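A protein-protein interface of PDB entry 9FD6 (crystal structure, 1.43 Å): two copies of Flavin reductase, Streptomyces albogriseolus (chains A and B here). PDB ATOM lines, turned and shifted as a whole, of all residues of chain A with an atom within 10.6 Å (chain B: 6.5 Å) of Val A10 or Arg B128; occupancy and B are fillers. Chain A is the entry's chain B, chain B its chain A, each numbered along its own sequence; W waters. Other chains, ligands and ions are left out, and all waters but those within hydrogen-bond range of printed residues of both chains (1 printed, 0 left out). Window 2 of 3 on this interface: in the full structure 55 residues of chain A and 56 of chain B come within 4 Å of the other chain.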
ATOM      1  N   VAL A  10     -27.824  10.725  28.154  1.00  0.00           N
ATOM      2  CA  VAL A  10     -26.960  10.528  26.989  1.00  0.00           C
ATOM      3  C   VAL A  10     -25.716  11.415  27.111  1.00  0.00           C
ATOM      4  O   VAL A  10     -25.811  12.601  27.422  1.00  0.00           O
ATOM      5  CB  VAL A  10     -27.738  10.766  25.673  1.00  0.00           C
ATOM      6  CG1 VAL A  10     -26.789  10.904  24.500  1.00  0.00           C
ATOM      7  CG2 VAL A  10     -28.736   9.624  25.423  1.00  0.00           C
ATOM      8  N   THR A  11     -24.547  10.828  26.857  1.00  0.00           N
ATOM      9  CA  THR A  11     -23.265  11.481  27.097  1.00  0.00           C
ATOM     10  C   THR A  11     -22.324  11.131  25.955  1.00  0.00           C
ATOM     11  O   THR A  11     -22.221   9.962  25.576  1.00  0.00           O
ATOM     12  CB  THR A  11     -22.675  10.993  28.429  1.00  0.00           C
ATOM     13  OG1 THR A  11     -23.605  11.256  29.489  1.00  0.00           O
ATOM     14  CG2 THR A  11     -21.350  11.686  28.735  1.00  0.00           C
ATOM     15  N   THR A  12     -21.648  12.136  25.406  1.00  0.00           N
ATOM     16  CA  THR A  12     -20.690  11.883  24.336  1.00  0.00           C
ATOM     17  C   THR A  12     -19.417  11.236  24.887  1.00  0.00           C
ATOM     18  O   THR A  12     -19.089  11.347  26.071  1.00  0.00           O
ATOM     19  CB  THR A  12     -20.351  13.192  23.621  1.00  0.00           C
ATOM     20  OG1 THR A  12     -19.771  12.907  22.343  1.00  0.00           O
ATOM     21  CG2 THR A  12     -19.365  14.024  24.445  1.00  0.00           C
ATOM     22  N   GLU A  13     -18.694  10.546  24.004  1.00  0.00           N
ATOM     23  CA  GLU A  13     -17.435   9.927  24.394  1.00  0.00           C
ATOM     24  C   GLU A  13     -16.319  10.974  24.436  1.00  0.00           C
ATOM     25  O   GLU A  13     -16.383  12.024  23.786  1.00  0.00           O
ATOM     26  CB  GLU A  13     -17.038   8.813  23.418  1.00  0.00           C
ATOM     27  CG  GLU A  13     -18.162   7.838  23.030  1.00  0.00           C
ATOM     28  CD  GLU A  13     -18.477   6.818  24.109  1.00  0.00           C
ATOM     29  OE1 GLU A  13     -17.748   6.783  25.130  1.00  0.00           O
ATOM     30  OE2 GLU A  13     -19.453   6.050  23.927  1.00  0.00           O
ATOM     31  N   HIS A  16     -14.598  11.976  21.030  1.00  0.00           N
ATOM     32  CA  HIS A  16     -15.410  12.870  20.216  1.00  0.00           C
ATOM     33  C   HIS A  16     -15.354  14.287  20.761  1.00  0.00           C
ATOM     34  O   HIS A  16     -15.335  15.258  19.996  1.00  0.00           O
ATOM     35  CB  HIS A  16     -16.847  12.367  20.187  1.00  0.00           C
ATOM     36  CG  HIS A  16     -16.998  11.030  19.543  1.00  0.00           C
ATOM     37  ND1 HIS A  16     -16.132  10.572  18.574  1.00  0.00           N
ATOM     38  CD2 HIS A  16     -17.908  10.047  19.735  1.00  0.00           C
ATOM     39  CE1 HIS A  16     -16.507   9.364  18.190  1.00  0.00           C
ATOM     40  NE2 HIS A  16     -17.582   9.024  18.878  1.00  0.00           N
ATOM     41  N   TYR A  17     -15.311  14.422  22.087  1.00  0.00           N
ATOM     42  CA  TYR A  17     -15.202  15.745  22.693  1.00  0.00           C
ATOM     43  C   TYR A  17     -13.843  16.382  22.413  1.00  0.00           C
ATOM     44  O   TYR A  17     -13.762  17.573  22.085  1.00  0.00           O
ATOM     45  CB  TYR A  17     -15.461  15.630  24.193  1.00  0.00           C
ATOM     46  CG  TYR A  17     -15.289  16.918  24.922  1.00  0.00           C
ATOM     47  CD1 TYR A  17     -16.306  17.859  24.960  1.00  0.00           C
ATOM     48  CD2 TYR A  17     -14.103  17.202  25.568  1.00  0.00           C
ATOM     49  CE1 TYR A  17     -16.139  19.040  25.620  1.00  0.00           C
ATOM     50  CE2 TYR A  17     -13.930  18.381  26.246  1.00  0.00           C
ATOM     51  CZ  TYR A  17     -14.952  19.296  26.269  1.00  0.00           C
ATOM     52  OH  TYR A  17     -14.790  20.490  26.920  1.00  0.00           O
ATOM     53  N   VAL A 135     -14.724  21.869  38.663  1.00  0.00           N
ATOM     54  CA  VAL A 135     -15.551  21.212  37.653  1.00  0.00           C
ATOM     55  C   VAL A 135     -14.792  19.973  37.221  1.00  0.00           C
ATOM     56  O   VAL A 135     -13.736  20.066  36.583  1.00  0.00           O
ATOM     57  CB  VAL A 135     -15.850  22.147  36.468  1.00  0.00           C
ATOM     58  CG1 VAL A 135     -14.581  22.776  35.923  1.00  0.00           C
ATOM     59  CG2 VAL A 135     -16.597  21.384  35.377  1.00  0.00           C
ATOM     60  N   ARG B  76     -32.497  24.726  30.153  1.00  0.00           N
ATOM     61  CA  ARG B  76     -31.390  23.957  30.732  1.00  0.00           C
ATOM     62  C   ARG B  76     -30.609  23.177  29.678  1.00  0.00           C
ATOM     63  O   ARG B  76     -29.973  22.162  29.976  1.00  0.00           O
ATOM     64  CB  ARG B  76     -31.852  23.052  31.875  1.00  0.00           C
ATOM     65  CG  ARG B  76     -32.575  23.798  32.992  1.00  0.00           C
ATOM     66  CD  ARG B  76     -31.830  25.058  33.482  1.00  0.00           C
ATOM     67  NE  ARG B  76     -30.659  24.762  34.303  1.00  0.00           N
ATOM     68  CZ  ARG B  76     -29.961  25.673  34.971  1.00  0.00           C
ATOM     69  NH1 ARG B  76     -30.235  26.966  34.868  1.00  0.00           N
ATOM     70  NH2 ARG B  76     -28.981  25.278  35.781  1.00  0.00           N
ATOM     71  N   GLY B  77     -30.623  23.676  28.449  1.00  0.00           N
ATOM     72  CA  GLY B  77     -29.843  23.075  27.385  1.00  0.00           C
ATOM     73  C   GLY B  77     -29.507  24.099  26.326  1.00  0.00           C
ATOM     74  O   GLY B  77     -30.152  25.146  26.207  1.00  0.00           O
ATOM     75  N   PHE B  78     -28.480  23.778  25.550  1.00  0.00           N
ATOM     76  CA  PHE B  78     -28.057  24.668  24.486  1.00  0.00           C
ATOM     77  C   PHE B  78     -27.188  23.904  23.508  1.00  0.00           C
ATOM     78  O   PHE B  78     -26.636  22.849  23.833  1.00  0.00           O
ATOM     79  CB  PHE B  78     -27.307  25.893  25.022  1.00  0.00           C
ATOM     80  CG  PHE B  78     -26.047  25.580  25.800  1.00  0.00           C
ATOM     81  CD1 PHE B  78     -26.102  25.285  27.157  1.00  0.00           C
ATOM     82  CD2 PHE B  78     -24.807  25.656  25.188  1.00  0.00           C
ATOM     83  CE1 PHE B  78     -24.942  25.044  27.883  1.00  0.00           C
ATOM     84  CE2 PHE B  78     -23.639  25.404  25.906  1.00  0.00           C
ATOM     85  CZ  PHE B  78     -23.711  25.100  27.257  1.00  0.00           C
ATOM     86  N   GLU B 126     -24.569  19.396  21.457  1.00  0.00           N
ATOM     87  CA  GLU B 126     -25.739  19.604  22.292  1.00  0.00           C
ATOM     88  C   GLU B 126     -25.316  19.376  23.731  1.00  0.00           C
ATOM     89  O   GLU B 126     -24.687  18.357  24.042  1.00  0.00           O
ATOM     90  CB  GLU B 126     -26.867  18.641  21.932  1.00  0.00           C
ATOM     91  CG  GLU B 126     -27.316  18.771  20.496  1.00  0.00           C
ATOM     92  CD  GLU B 126     -28.661  18.125  20.236  1.00  0.00           C
ATOM     93  OE1 GLU B 126     -29.560  18.240  21.095  1.00  0.00           O
ATOM     94  OE2 GLU B 126     -28.819  17.502  19.167  1.00  0.00           O
ATOM     95  N   CYS B 127     -25.661  20.329  24.592  1.00  0.00           N
ATOM     96  CA  CYS B 127     -25.205  20.365  25.969  1.00  0.00           C
ATOM     97  C   CYS B 127     -26.382  20.495  26.924  1.00  0.00           C
ATOM     98  O   CYS B 127     -27.378  21.156  26.616  1.00  0.00           O
ATOM     99  CB  CYS B 127     -24.296  21.567  26.182  1.00  0.00           C
ATOM    100  SG  CYS B 127     -22.858  21.583  25.124  1.00  0.00           S
ATOM    101  N   ARG B 128     -26.253  19.851  28.084  1.00  0.00           N
ATOM    102  CA  ARG B 128     -27.128  20.072  29.224  1.00  0.00           C
ATOM    103  C   ARG B 128     -26.425  21.014  30.188  1.00  0.00           C
ATOM    104  O   ARG B 128     -25.234  20.848  30.466  1.00  0.00           O
ATOM    105  CB  ARG B 128     -27.390  18.769  29.977  1.00  0.00           C
ATOM    106  CG  ARG B 128     -28.230  17.776  29.230  1.00  0.00           C
ATOM    107  CD  ARG B 128     -28.536  16.575  30.104  1.00  0.00           C
ATOM    108  NE  ARG B 128     -27.330  15.805  30.383  1.00  0.00           N
ATOM    109  CZ  ARG B 128     -26.856  14.846  29.596  1.00  0.00           C
ATOM    110  NH1 ARG B 128     -27.495  14.473  28.499  1.00  0.00           N
ATOM    111  NH2 ARG B 128     -25.711  14.249  29.916  1.00  0.00           N
ATOM    112  N   VAL B 129     -27.162  21.996  30.702  1.00  0.00           N
ATOM    113  CA  VAL B 129     -26.601  22.893  31.704  1.00  0.00           C
ATOM    114  C   VAL B 129     -26.377  22.103  32.984  1.00  0.00           C
ATOM    115  O   VAL B 129     -27.322  21.549  33.559  1.00  0.00           O
ATOM    116  CB  VAL B 129     -27.524  24.093  31.948  1.00  0.00           C
ATOM    117  CG1 VAL B 129     -26.996  24.911  33.128  1.00  0.00           C
ATOM    118  CG2 VAL B 129     -27.638  24.943  30.676  1.00  0.00           C
ATOM    119  N   SER B 130     -25.124  22.035  33.429  1.00  0.00           N
ATOM    120  CA  SER B 130     -24.770  21.318  34.645  1.00  0.00           C
ATOM    121  C   SER B 130     -24.436  22.245  35.801  1.00  0.00           C
ATOM    122  O   SER B 130     -24.238  21.769  36.925  1.00  0.00           O
ATOM    123  CB  SER B 130     -23.584  20.382  34.379  1.00  0.00           C
ATOM    124  OG  SER B 130     -22.474  21.082  33.851  1.00  0.00           O
ATOM    125  N   GLY B 131     -24.369  23.543  35.556  1.00  0.00           N
ATOM    126  CA  GLY B 131     -24.152  24.501  36.611  1.00  0.00           C
ATOM    127  C   GLY B 131     -23.968  25.872  36.013  1.00  0.00           C
ATOM    128  O   GLY B 131     -23.730  26.003  34.808  1.00  0.00           O
ATOM    129  N   PHE B 142     -21.921  26.073  32.571  1.00  0.00           N
ATOM    130  CA  PHE B 142     -21.256  24.803  32.332  1.00  0.00           C
ATOM    131  C   PHE B 142     -22.180  23.886  31.545  1.00  0.00           C
ATOM    132  O   PHE B 142     -23.354  23.730  31.894  1.00  0.00           O
ATOM    133  CB  PHE B 142     -20.880  24.166  33.660  1.00  0.00           C
ATOM    134  CG  PHE B 142     -19.876  24.956  34.433  1.00  0.00           C
ATOM    135  CD1 PHE B 142     -18.524  24.775  34.203  1.00  0.00           C
ATOM    136  CD2 PHE B 142     -20.272  25.887  35.376  1.00  0.00           C
ATOM    137  CE1 PHE B 142     -17.582  25.492  34.910  1.00  0.00           C
ATOM    138  CE2 PHE B 142     -19.324  26.616  36.094  1.00  0.00           C
ATOM    139  CZ  PHE B 142     -17.980  26.420  35.854  1.00  0.00           C
ATOM    140  N   GLY B 143     -21.651  23.303  30.474  1.00  0.00           N
ATOM    141  CA  GLY B 143     -22.432  22.451  29.605  1.00  0.00           C
ATOM    142  C   GLY B 143     -21.831  21.067  29.496  1.00  0.00           C
ATOM    143  O   GLY B 143     -20.729  20.890  28.967  1.00  0.00           O
ATOM    144  N   GLU B 144     -22.538  20.075  30.020  1.00  0.00           N
ATOM    145  CA  GLU B 144     -22.129  18.689  29.856  1.00  0.00           C
ATOM    146  C   GLU B 144     -22.606  18.229  28.487  1.00  0.00           C
ATOM    147  O   GLU B 144     -23.802  18.298  28.178  1.00  0.00           O
ATOM    148  CB  GLU B 144     -22.686  17.820  30.979  1.00  0.00           C
ATOM    149  CG  GLU B 144     -21.905  17.988  32.283  1.00  0.00           C
ATOM    150  CD  GLU B 144     -22.410  17.125  33.432  1.00  0.00           C
ATOM    151  OE1 GLU B 144     -23.397  16.371  33.267  1.00  0.00           O
ATOM    152  OE2 GLU B 144     -21.796  17.196  34.513  1.00  0.00           O
ATOM    153  N   VAL B 145     -21.668  17.789  27.663  1.00  0.00           N
ATOM    154  CA  VAL B 145     -21.952  17.541  26.258  1.00  0.00           C
ATOM    155  C   VAL B 145     -22.660  16.201  26.112  1.00  0.00           C
ATOM    156  O   VAL B 145     -22.148  15.163  26.548  1.00  0.00           O
ATOM    157  CB  VAL B 145     -20.665  17.587  25.424  1.00  0.00           C
ATOM    158  CG1 VAL B 145     -20.988  17.332  23.970  1.00  0.00           C
ATOM    159  CG2 VAL B 145     -19.973  18.941  25.585  1.00  0.00           C
ATOM    160  N   ALA B 146     -23.839  16.229  25.491  1.00  0.00           N
ATOM    161  CA  ALA B 146     -24.666  15.051  25.276  1.00  0.00           C
ATOM    162  C   ALA B 146     -24.475  14.433  23.903  1.00  0.00           C
ATOM    163  O   ALA B 146     -24.552  13.212  23.770  1.00  0.00           O
ATOM    164  CB  ALA B 146     -26.144  15.424  25.428  1.00  0.00           C
ATOM    165  N   ARG B 147     -24.258  15.245  22.873  1.00  0.00           N
ATOM    166  CA  ARG B 147     -24.153  14.751  21.511  1.00  0.00           C
ATOM    167  C   ARG B 147     -23.273  15.702  20.725  1.00  0.00           C
ATOM    168  O   ARG B 147     -23.386  16.922  20.868  1.00  0.00           O
ATOM    169  CB  ARG B 147     -25.523  14.699  20.827  1.00  0.00           C
ATOM    170  CG  ARG B 147     -25.505  14.001  19.478  1.00  0.00           C
ATOM    171  CD  ARG B 147     -26.883  13.982  18.851  1.00  0.00           C
ATOM    172  NE  ARG B 147     -27.274  15.300  18.373  1.00  0.00           N
ATOM    173  CZ  ARG B 147     -26.905  15.809  17.206  1.00  0.00           C
ATOM    174  NH1 ARG B 147     -26.146  15.126  16.364  1.00  0.00           N
ATOM    175  NH2 ARG B 147     -27.314  17.028  16.873  1.00  0.00           N
HETATM  176  O   HOH W   1     -22.654  13.805  31.063  1.00  0.00           O
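No position is printed for both chains.
Of the 8 pairs that touch across the chains among the printed residues, none has its exchanged pair printed and touching as well.
The guanidinium group (NH1) of Arg B128 sits at hydrogen-bond distance from the backbone carbonyl oxygen (O) of Val A10, at 2.7 Å.
O of Val B145 is in hydrogen-bond range of N of Thr A12, at 3.3 Å.
Of the 15 printed residues of chain B, 3 touch a printed residue of chain A.
Printed residues of chain B that touch a printed residue of chain A: Arg B128, Val B145 and Ala B146.
Along chain B the printed residues that touch a printed residue of chain A span positions 128 to 146.
Printed residues of chain A that touch a printed residue of chain B: Val A10, Thr A11, Thr A12 and Tyr A17.
Hydrophobic or aromatic side chains of chain A within 4 Å of the printed part of chain B: Val A10 and Tyr A17.
Among the printed residues, no Asp or Glu carboxylate lies within 4 Å of a Lys or Arg side-chain nitrogen of the other chain.
The backbone NH (N) of Ala B146 lies within hydrogen-bond range of the backbone carbonyl oxygen (O) of Glu B126 (2.7 Å).
The backbone carbonyl oxygen (O) of Arg B128 sits at hydrogen-bond distance from the backbone NH (N) of Glu B144 (2.8 Å).
Among the printed residues, pairs that only touch across the chains: Val A10 with Ala B146, Thr A11 with Arg B128, Thr A11 with Val B145, Thr A11 with Ala B146, Thr A12 with Ala B146 and Tyr A17 with Val B145.
Of chain B, only Arg B128 (2.7 Å) and Ala B146 (3.3 Å) come within 4 Å of Val A10.
Printed residues of chain B within 4 Å of Thr A11: Arg B128, Val B145 and Ala B146.
Printed residues of chain B within 4 Å of Thr A12: Val B145 and Ala B146.
Printed residues of chain B within 4 Å of Tyr A17: Val B145.
Arg B128 touches two residues of chain A.
No residue of chain A comes within 4 Å of Gly B143.
Glu B144 touches none of the printed residues of chain A.
Printed residues of chain A within 4 Å of Val B145: Thr A11, Thr A12 and Tyr A17.
Ala B146 touches three residues of chain A.
Water W1 lies within hydrogen-bond range of the side-chain hydroxyl of Thr A11 (3.1 Å), the guanidinium group of Arg B128 (3.3 Å) and the side-chain carboxylate of Glu B144 (3.5 Å).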
